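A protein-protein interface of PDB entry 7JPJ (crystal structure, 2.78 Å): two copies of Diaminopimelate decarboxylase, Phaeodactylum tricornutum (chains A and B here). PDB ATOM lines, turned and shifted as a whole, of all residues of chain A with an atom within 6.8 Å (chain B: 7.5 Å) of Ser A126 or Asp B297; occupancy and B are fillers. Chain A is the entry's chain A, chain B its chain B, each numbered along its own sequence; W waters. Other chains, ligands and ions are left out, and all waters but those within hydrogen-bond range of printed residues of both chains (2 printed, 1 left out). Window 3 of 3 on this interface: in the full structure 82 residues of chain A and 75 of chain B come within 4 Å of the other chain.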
ATOM      1  N   GLN A 104      15.296   7.547   8.450  1.00  0.00           N
ATOM      2  CA  GLN A 104      14.157   7.190   9.285  1.00  0.00           C
ATOM      3  C   GLN A 104      14.189   7.894  10.633  1.00  0.00           C
ATOM      4  O   GLN A 104      13.144   8.021  11.277  1.00  0.00           O
ATOM      5  CB  GLN A 104      14.114   5.676   9.512  1.00  0.00           C
ATOM      6  CG  GLN A 104      13.692   4.861   8.299  1.00  0.00           C
ATOM      7  CD  GLN A 104      12.191   4.862   8.087  1.00  0.00           C
ATOM      8  OE1 GLN A 104      11.625   5.837   7.597  1.00  0.00           O
ATOM      9  NE2 GLN A 104      11.537   3.768   8.457  1.00  0.00           N
ATOM     10  N   GLU A 105      15.361   8.356  11.064  1.00  0.00           N
ATOM     11  CA  GLU A 105      15.559   8.959  12.381  1.00  0.00           C
ATOM     12  C   GLU A 105      16.273  10.293  12.185  1.00  0.00           C
ATOM     13  O   GLU A 105      17.489  10.329  11.968  1.00  0.00           O
ATOM     14  CB  GLU A 105      16.358   8.025  13.287  1.00  0.00           C
ATOM     15  CG  GLU A 105      16.813   8.629  14.604  1.00  0.00           C
ATOM     16  CD  GLU A 105      17.717   7.688  15.381  1.00  0.00           C
ATOM     17  OE1 GLU A 105      17.799   6.499  15.007  1.00  0.00           O
ATOM     18  OE2 GLU A 105      18.345   8.134  16.367  1.00  0.00           O
ATOM     19  N   LEU A 106      15.521  11.382  12.250  1.00  0.00           N
ATOM     20  CA  LEU A 106      16.111  12.709  12.115  1.00  0.00           C
ATOM     21  C   LEU A 106      17.002  12.993  13.318  1.00  0.00           C
ATOM     22  O   LEU A 106      16.513  12.977  14.454  1.00  0.00           O
ATOM     23  CB  LEU A 106      15.018  13.768  11.992  1.00  0.00           C
ATOM     24  CG  LEU A 106      15.433  15.134  11.442  1.00  0.00           C
ATOM     25  CD1 LEU A 106      16.127  14.989  10.100  1.00  0.00           C
ATOM     26  CD2 LEU A 106      14.229  16.054  11.325  1.00  0.00           C
ATOM     27  N   CYS A 123      11.214  13.097   5.361  1.00  0.00           N
ATOM     28  CA  CYS A 123      10.671  11.768   5.120  1.00  0.00           C
ATOM     29  C   CYS A 123       9.396  11.480   5.900  1.00  0.00           C
ATOM     30  O   CYS A 123       8.828  10.395   5.747  1.00  0.00           O
ATOM     31  CB  CYS A 123      11.728  10.707   5.442  1.00  0.00           C
ATOM     32  SG  CYS A 123      13.170  10.768   4.340  1.00  0.00           S
ATOM     33  N   SER A 124       8.930  12.411   6.728  1.00  0.00           N
ATOM     34  CA  SER A 124       7.658  12.257   7.420  1.00  0.00           C
ATOM     35  C   SER A 124       7.133  13.642   7.764  1.00  0.00           C
ATOM     36  O   SER A 124       7.850  14.641   7.672  1.00  0.00           O
ATOM     37  CB  SER A 124       7.794  11.400   8.681  1.00  0.00           C
ATOM     38  OG  SER A 124       8.576  12.054   9.666  1.00  0.00           O
ATOM     39  N   VAL A 125       5.860  13.688   8.159  1.00  0.00           N
ATOM     40  CA  VAL A 125       5.273  14.950   8.598  1.00  0.00           C
ATOM     41  C   VAL A 125       6.046  15.508   9.786  1.00  0.00           C
ATOM     42  O   VAL A 125       6.335  16.709   9.848  1.00  0.00           O
ATOM     43  CB  VAL A 125       3.780  14.757   8.922  1.00  0.00           C
ATOM     44  CG1 VAL A 125       3.222  15.972   9.653  1.00  0.00           C
ATOM     45  CG2 VAL A 125       2.996  14.491   7.644  1.00  0.00           C
ATOM     46  N   SER A 126       6.421  14.637  10.730  1.00  0.00           N
ATOM     47  CA  SER A 126       7.142  15.075  11.923  1.00  0.00           C
ATOM     48  C   SER A 126       8.455  15.758  11.565  1.00  0.00           C
ATOM     49  O   SER A 126       8.830  16.760  12.185  1.00  0.00           O
ATOM     50  CB  SER A 126       7.414  13.880  12.834  1.00  0.00           C
ATOM     51  OG  SER A 126       6.386  12.917  12.717  1.00  0.00           O
ATOM     52  N   GLN A 127       9.178  15.223  10.578  1.00  0.00           N
ATOM     53  CA  GLN A 127      10.462  15.809  10.207  1.00  0.00           C
ATOM     54  C   GLN A 127      10.278  17.159   9.533  1.00  0.00           C
ATOM     55  O   GLN A 127      11.042  18.097   9.789  1.00  0.00           O
ATOM     56  CB  GLN A 127      11.232  14.861   9.293  1.00  0.00           C
ATOM     57  CG  GLN A 127      11.683  13.586   9.964  1.00  0.00           C
ATOM     58  CD  GLN A 127      12.557  12.743   9.065  1.00  0.00           C
ATOM     59  OE1 GLN A 127      12.687  13.019   7.872  1.00  0.00           O
ATOM     60  NE2 GLN A 127      13.170  11.710   9.633  1.00  0.00           N
ATOM     61  N   LEU A 128       9.275  17.272   8.662  1.00  0.00           N
ATOM     62  CA  LEU A 128       8.999  18.548   8.018  1.00  0.00           C
ATOM     63  C   LEU A 128       8.633  19.610   9.046  1.00  0.00           C
ATOM     64  O   LEU A 128       9.100  20.752   8.967  1.00  0.00           O
ATOM     65  CB  LEU A 128       7.879  18.378   6.993  1.00  0.00           C
ATOM     66  CG  LEU A 128       7.716  19.477   5.944  1.00  0.00           C
ATOM     67  CD1 LEU A 128       9.007  19.661   5.167  1.00  0.00           C
ATOM     68  CD2 LEU A 128       6.566  19.144   5.011  1.00  0.00           C
ATOM     69  N   GLU A 129       7.808  19.248  10.030  1.00  0.00           N
ATOM     70  CA  GLU A 129       7.395  20.221  11.035  1.00  0.00           C
ATOM     71  C   GLU A 129       8.570  20.655  11.902  1.00  0.00           C
ATOM     72  O   GLU A 129       8.692  21.839  12.239  1.00  0.00           O
ATOM     73  CB  GLU A 129       6.272  19.642  11.895  1.00  0.00           C
ATOM     74  CG  GLU A 129       4.935  19.547  11.178  1.00  0.00           C
ATOM     75  CD  GLU A 129       3.886  18.827  12.003  1.00  0.00           C
ATOM     76  OE1 GLU A 129       4.267  18.091  12.938  1.00  0.00           O
ATOM     77  OE2 GLU A 129       2.683  19.002  11.718  1.00  0.00           O
ATOM     78  N   ARG A 130       9.445  19.715  12.273  1.00  0.00           N
ATOM     79  CA  ARG A 130      10.639  20.080  13.031  1.00  0.00           C
ATOM     80  C   ARG A 130      11.550  20.988  12.213  1.00  0.00           C
ATOM     81  O   ARG A 130      12.126  21.946  12.743  1.00  0.00           O
ATOM     82  CB  ARG A 130      11.386  18.821  13.475  1.00  0.00           C
ATOM     83  CG  ARG A 130      10.639  17.978  14.505  1.00  0.00           C
ATOM     84  CD  ARG A 130      11.415  16.720  14.863  1.00  0.00           C
ATOM     85  NE  ARG A 130      12.691  17.035  15.497  1.00  0.00           N
ATOM     86  CZ  ARG A 130      13.652  16.147  15.732  1.00  0.00           C
ATOM     87  NH1 ARG A 130      13.486  14.877  15.385  1.00  0.00           N
ATOM     88  NH2 ARG A 130      14.782  16.532  16.313  1.00  0.00           N
ATOM     89  N   PHE A 131      11.688  20.705  10.915  1.00  0.00           N
ATOM     90  CA  PHE A 131      12.455  21.583  10.038  1.00  0.00           C
ATOM     91  C   PHE A 131      11.797  22.953   9.932  1.00  0.00           C
ATOM     92  O   PHE A 131      12.469  23.988  10.024  1.00  0.00           O
ATOM     93  CB  PHE A 131      12.593  20.938   8.657  1.00  0.00           C
ATOM     94  CG  PHE A 131      13.532  21.661   7.736  1.00  0.00           C
ATOM     95  CD1 PHE A 131      14.883  21.356   7.725  1.00  0.00           C
ATOM     96  CD2 PHE A 131      13.063  22.637   6.872  1.00  0.00           C
ATOM     97  CE1 PHE A 131      15.749  22.014   6.871  1.00  0.00           C
ATOM     98  CE2 PHE A 131      13.923  23.298   6.022  1.00  0.00           C
ATOM     99  CZ  PHE A 131      15.268  22.986   6.021  1.00  0.00           C
ATOM    100  N   ILE A 176       6.356  10.119   2.994  1.00  0.00           N
ATOM    101  CA  ILE A 176       5.052  10.612   3.418  1.00  0.00           C
ATOM    102  C   ILE A 176       3.982  10.010   2.523  1.00  0.00           C
ATOM    103  O   ILE A 176       4.141   9.942   1.299  1.00  0.00           O
ATOM    104  CB  ILE A 176       5.010  12.151   3.378  1.00  0.00           C
ATOM    105  CG1 ILE A 176       6.216  12.738   4.114  1.00  0.00           C
ATOM    106  CG2 ILE A 176       3.714  12.671   3.975  1.00  0.00           C
ATOM    107  CD1 ILE A 176       6.210  14.250   4.187  1.00  0.00           C
ATOM    108  N   ILE A 189       1.524  22.588   5.897  1.00  0.00           N
ATOM    109  CA  ILE A 189       2.723  22.693   6.721  1.00  0.00           C
ATOM    110  C   ILE A 189       3.761  23.574   6.038  1.00  0.00           C
ATOM    111  O   ILE A 189       4.462  24.356   6.692  1.00  0.00           O
ATOM    112  CB  ILE A 189       3.278  21.291   7.029  1.00  0.00           C
ATOM    113  CG1 ILE A 189       2.207  20.432   7.704  1.00  0.00           C
ATOM    114  CG2 ILE A 189       4.518  21.386   7.905  1.00  0.00           C
ATOM    115  CD1 ILE A 189       2.456  18.942   7.603  1.00  0.00           C
ATOM    116  N   LYS B 294      13.283   4.405  22.118  1.00  0.00           N
ATOM    117  CA  LYS B 294      12.330   5.505  22.120  1.00  0.00           C
ATOM    118  C   LYS B 294      11.552   5.519  20.810  1.00  0.00           C
ATOM    119  O   LYS B 294      12.120   5.286  19.736  1.00  0.00           O
ATOM    120  CB  LYS B 294      13.051   6.850  22.320  1.00  0.00           C
ATOM    121  CG  LYS B 294      12.157   8.079  22.169  1.00  0.00           C
ATOM    122  CD  LYS B 294      12.950   9.379  22.261  1.00  0.00           C
ATOM    123  CE  LYS B 294      13.944   9.509  21.120  1.00  0.00           C
ATOM    124  NZ  LYS B 294      14.734  10.768  21.215  1.00  0.00           N
ATOM    125  N   VAL B 295      10.250   5.787  20.904  1.00  0.00           N
ATOM    126  CA  VAL B 295       9.401   5.975  19.728  1.00  0.00           C
ATOM    127  C   VAL B 295       9.644   7.394  19.219  1.00  0.00           C
ATOM    128  O   VAL B 295       9.079   8.358  19.739  1.00  0.00           O
ATOM    129  CB  VAL B 295       7.923   5.733  20.044  1.00  0.00           C
ATOM    130  CG1 VAL B 295       7.066   6.009  18.817  1.00  0.00           C
ATOM    131  CG2 VAL B 295       7.720   4.309  20.532  1.00  0.00           C
ATOM    132  N   GLN B 296      10.484   7.526  18.192  1.00  0.00           N
ATOM    133  CA  GLN B 296      10.866   8.836  17.685  1.00  0.00           C
ATOM    134  C   GLN B 296      10.046   9.291  16.482  1.00  0.00           C
ATOM    135  O   GLN B 296      10.213  10.432  16.040  1.00  0.00           O
ATOM    136  CB  GLN B 296      12.360   8.853  17.336  1.00  0.00           C
ATOM    137  CG  GLN B 296      12.785   7.780  16.360  1.00  0.00           C
ATOM    138  CD  GLN B 296      12.920   8.307  14.948  1.00  0.00           C
ATOM    139  OE1 GLN B 296      12.978   9.519  14.727  1.00  0.00           O
ATOM    140  NE2 GLN B 296      12.967   7.398  13.981  1.00  0.00           N
ATOM    141  N   ASP B 297       9.161   8.444  15.953  1.00  0.00           N
ATOM    142  CA  ASP B 297       8.235   8.864  14.907  1.00  0.00           C
ATOM    143  C   ASP B 297       7.069   7.885  14.860  1.00  0.00           C
ATOM    144  O   ASP B 297       7.157   6.761  15.358  1.00  0.00           O
ATOM    145  CB  ASP B 297       8.920   8.955  13.537  1.00  0.00           C
ATOM    146  CG  ASP B 297       8.225   9.932  12.601  1.00  0.00           C
ATOM    147  OD1 ASP B 297       7.029  10.222  12.820  1.00  0.00           O
ATOM    148  OD2 ASP B 297       8.874  10.406  11.642  1.00  0.00           O
ATOM    149  N   LYS B 298       5.972   8.334  14.244  1.00  0.00           N
ATOM    150  CA  LYS B 298       4.746   7.540  14.173  1.00  0.00           C
ATOM    151  C   LYS B 298       3.967   7.986  12.942  1.00  0.00           C
ATOM    152  O   LYS B 298       3.474   9.117  12.903  1.00  0.00           O
ATOM    153  CB  LYS B 298       3.921   7.713  15.444  1.00  0.00           C
ATOM    154  CG  LYS B 298       2.554   7.052  15.408  1.00  0.00           C
ATOM    155  CD  LYS B 298       1.838   7.214  16.737  1.00  0.00           C
ATOM    156  CE  LYS B 298       0.415   6.694  16.662  1.00  0.00           C
ATOM    157  NZ  LYS B 298      -0.294   6.823  17.962  1.00  0.00           N
ATOM    158  N   VAL B 299       3.844   7.104  11.952  1.00  0.00           N
ATOM    159  CA  VAL B 299       3.259   7.452  10.663  1.00  0.00           C
ATOM    160  C   VAL B 299       2.095   6.510  10.364  1.00  0.00           C
ATOM    161  O   VAL B 299       1.923   5.472  11.003  1.00  0.00           O
ATOM    162  CB  VAL B 299       4.299   7.422   9.526  1.00  0.00           C
ATOM    163  CG1 VAL B 299       5.438   8.380   9.831  1.00  0.00           C
ATOM    164  CG2 VAL B 299       4.828   6.014   9.321  1.00  0.00           C
ATOM    165  N   HIS B 300       1.294   6.887   9.368  1.00  0.00           N
ATOM    166  CA  HIS B 300       0.076   6.166   9.027  1.00  0.00           C
ATOM    167  C   HIS B 300       0.013   5.908   7.527  1.00  0.00           C
ATOM    168  O   HIS B 300       0.731   6.523   6.735  1.00  0.00           O
ATOM    169  CB  HIS B 300      -1.181   6.940   9.460  1.00  0.00           C
ATOM    170  CG  HIS B 300      -1.372   7.017  10.944  1.00  0.00           C
ATOM    171  ND1 HIS B 300      -0.554   7.767  11.764  1.00  0.00           N
ATOM    172  CD2 HIS B 300      -2.295   6.446  11.756  1.00  0.00           C
ATOM    173  CE1 HIS B 300      -0.963   7.651  13.016  1.00  0.00           C
ATOM    174  NE2 HIS B 300      -2.018   6.856  13.038  1.00  0.00           N
ATOM    175  N   PHE B 309       2.432   2.839  12.006  1.00  0.00           N
ATOM    176  CA  PHE B 309       3.823   2.464  12.215  1.00  0.00           C
ATOM    177  C   PHE B 309       4.416   3.231  13.388  1.00  0.00           C
ATOM    178  O   PHE B 309       4.166   4.429  13.551  1.00  0.00           O
ATOM    179  CB  PHE B 309       4.662   2.728  10.959  1.00  0.00           C
ATOM    180  CG  PHE B 309       4.250   1.911   9.768  1.00  0.00           C
ATOM    181  CD1 PHE B 309       3.247   2.353   8.921  1.00  0.00           C
ATOM    182  CD2 PHE B 309       4.866   0.702   9.496  1.00  0.00           C
ATOM    183  CE1 PHE B 309       2.864   1.601   7.829  1.00  0.00           C
ATOM    184  CE2 PHE B 309       4.489  -0.053   8.404  1.00  0.00           C
ATOM    185  CZ  PHE B 309       3.487   0.398   7.570  1.00  0.00           C
ATOM    186  N   LEU B 310       5.205   2.534  14.198  1.00  0.00           N
ATOM    187  CA  LEU B 310       6.047   3.151  15.214  1.00  0.00           C
ATOM    188  C   LEU B 310       7.496   3.016  14.765  1.00  0.00           C
ATOM    189  O   LEU B 310       7.974   1.901  14.528  1.00  0.00           O
ATOM    190  CB  LEU B 310       5.841   2.498  16.581  1.00  0.00           C
ATOM    191  CG  LEU B 310       4.444   2.590  17.202  1.00  0.00           C
ATOM    192  CD1 LEU B 310       4.475   2.108  18.645  1.00  0.00           C
ATOM    193  CD2 LEU B 310       3.886   4.005  17.107  1.00  0.00           C
ATOM    194  N   LYS B 311       8.184   4.144  14.632  1.00  0.00           N
ATOM    195  CA  LYS B 311       9.588   4.161  14.238  1.00  0.00           C
ATOM    196  C   LYS B 311      10.439   4.257  15.497  1.00  0.00           C
ATOM    197  O   LYS B 311      10.406   5.273  16.199  1.00  0.00           O
ATOM    198  CB  LYS B 311       9.881   5.321  13.292  1.00  0.00           C
ATOM    199  CG  LYS B 311       9.197   5.235  11.940  1.00  0.00           C
ATOM    200  CD  LYS B 311       9.750   6.297  11.001  1.00  0.00           C
ATOM    201  CE  LYS B 311       9.020   6.316   9.671  1.00  0.00           C
ATOM    202  NZ  LYS B 311       9.615   7.322   8.743  1.00  0.00           N
ATOM    203  N   LEU B 312      11.199   3.206  15.781  1.00  0.00           N
ATOM    204  CA  LEU B 312      12.099   3.238  16.921  1.00  0.00           C
ATOM    205  C   LEU B 312      13.409   3.923  16.544  1.00  0.00           C
ATOM    206  O   LEU B 312      13.737   4.090  15.368  1.00  0.00           O
ATOM    207  CB  LEU B 312      12.382   1.823  17.431  1.00  0.00           C
ATOM    208  CG  LEU B 312      11.203   1.026  17.991  1.00  0.00           C
ATOM    209  CD1 LEU B 312      11.665  -0.354  18.430  1.00  0.00           C
ATOM    210  CD2 LEU B 312      10.528   1.766  19.139  1.00  0.00           C
ATOM    211  N   ASP B 313      14.159   4.334  17.565  1.00  0.00           N
ATOM    212  CA  ASP B 313      15.529   4.783  17.364  1.00  0.00           C
ATOM    213  C   ASP B 313      16.527   3.639  17.494  1.00  0.00           C
ATOM    214  O   ASP B 313      17.726   3.883  17.669  1.00  0.00           O
ATOM    215  CB  ASP B 313      15.869   5.924  18.328  1.00  0.00           C
ATOM    216  CG  ASP B 313      15.976   5.470  19.773  1.00  0.00           C
ATOM    217  OD1 ASP B 313      15.354   4.448  20.132  1.00  0.00           O
ATOM    218  OD2 ASP B 313      16.677   6.148  20.556  1.00  0.00           O
ATOM    219  N   VAL B 353       8.825  -0.664  13.401  1.00  0.00           N
ATOM    220  CA  VAL B 353       9.925  -0.750  12.451  1.00  0.00           C
ATOM    221  C   VAL B 353      11.140  -0.040  13.033  1.00  0.00           C
ATOM    222  O   VAL B 353      11.018   0.866  13.862  1.00  0.00           O
ATOM    223  CB  VAL B 353       9.552  -0.148  11.078  1.00  0.00           C
ATOM    224  CG1 VAL B 353       8.302  -0.813  10.528  1.00  0.00           C
ATOM    225  CG2 VAL B 353       9.364   1.357  11.185  1.00  0.00           C
ATOM    226  N   ALA B 381       0.857   4.797  21.795  1.00  0.00           N
ATOM    227  CA  ALA B 381       2.180   5.396  21.892  1.00  0.00           C
ATOM    228  C   ALA B 381       2.181   6.798  21.301  1.00  0.00           C
ATOM    229  O   ALA B 381       1.741   7.001  20.164  1.00  0.00           O
ATOM    230  CB  ALA B 381       3.222   4.529  21.184  1.00  0.00           C
ATOM    231  N   ALA B 382       2.667   7.757  22.081  1.00  0.00           N
ATOM    232  CA  ALA B 382       2.994   9.087  21.594  1.00  0.00           C
ATOM    233  C   ALA B 382       4.497   9.172  21.354  1.00  0.00           C
ATOM    234  O   ALA B 382       5.280   8.445  21.971  1.00  0.00           O
ATOM    235  CB  ALA B 382       2.556  10.161  22.589  1.00  0.00           C
ATOM    236  N   VAL B 383       4.893  10.052  20.433  1.00  0.00           N
ATOM    237  CA  VAL B 383       6.311  10.212  20.134  1.00  0.00           C
ATOM    238  C   VAL B 383       7.037  10.655  21.394  1.00  0.00           C
ATOM    239  O   VAL B 383       6.607  11.583  22.089  1.00  0.00           O
ATOM    240  CB  VAL B 383       6.507  11.204  18.979  1.00  0.00           C
ATOM    241  CG1 VAL B 383       7.854  11.906  19.093  1.00  0.00           C
ATOM    242  CG2 VAL B 383       6.399  10.479  17.651  1.00  0.00           C
ATOM    243  N   GLY B 384       8.140   9.976  21.702  1.00  0.00           N
ATOM    244  CA  GLY B 384       8.864  10.191  22.933  1.00  0.00           C
ATOM    245  C   GLY B 384       8.657   9.111  23.971  1.00  0.00           C
ATOM    246  O   GLY B 384       9.418   9.056  24.944  1.00  0.00           O
HETATM  247  O   HOH W   1       7.203   8.559   7.073  1.00  0.00           O
HETATM  248  O   HOH W   2      12.969  10.984  12.354  1.00  0.00           O
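No position is printed for both chains. Of the 7 pairs that touch across the chains among the printed residues, none has its exchanged pair printed and touching as well.
OG of Ser A124 sits at hydrogen-bond distance from N of Gln A127, 3.4 Å away. The backbone NH (N) of Lys B294 sits at hydrogen-bond distance from the side-chain carboxylate (OD1) of Asp B313 (2.9 Å). O of Lys B311 sits at hydrogen-bond distance from N of Gln B296. N of Lys B311 sits at hydrogen-bond distance from O of Asp B297. O of Val B299 sits at hydrogen-bond distance from N of Phe B309, at 2.9 Å.
Of the 17 printed residues of chain B, 5 touch a printed residue of chain A. Among the printed residues, no Asp or Glu carboxylate lies within 4 Å of a Lys or Arg side-chain nitrogen of the other chain.
The backbone carbonyl oxygen (O) of Gln A104 is in hydrogen-bond range of the side-chain amide nitrogen (NE2) of Gln B296 (2.8 Å). The side-chain amide oxygen of Gln A104 is in hydrogen-bond range of the side-chain amino group of Lys B311 (2.7 Å). The side-chain carboxylate (OD2) of Asp B297 sits at hydrogen-bond distance from the side-chain hydroxyl (OG) of Ser A124 (2.6 Å). OG of Ser A126 lies within hydrogen-bond range of OD1 of Asp B297 (2.8 Å).
Water W2 lies within hydrogen-bond range of the backbone NH of Leu A106 (2.6 Å), the side-chain amide oxygen of Gln B296 (2.8 Å), the side-chain amide nitrogen of Gln A127 (2.8 Å) and the backbone carbonyl oxygen of Gln A104 (3.2 Å). Water W1 lies within hydrogen-bond range of the backbone carbonyl oxygen (O) of Cys A123 and the side-chain amino group (NZ) of Lys B311.
Among the printed residues, merely in contact across the chains: Glu A105 with Gln B296 (3.4 Å), Glu A105 with Asp B313 (3.7 Å) and Ser A124 with Val B299 (3.999 Å).
Of chain B, only Asp B297 (2.8 Å) comes within 4 Å of Ser A126. Of chain A, only Ser A124 (2.6 Å) and Ser A126 (2.8 Å) come within 4 Å of Asp B297. Of the printed residues of chain A, Lys B311 touches Gln A104 (2.7 Å). Printed residues of chain B within 4 Å of Ser A124: Asp B297 and Val B299. Leu A128 touches none of the printed residues of chain B. Ala B382 touches none of the printed residues of chain A. The nearest residue of chain B that does not touch Ser A126 is Lys B298 (4.8 Å).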
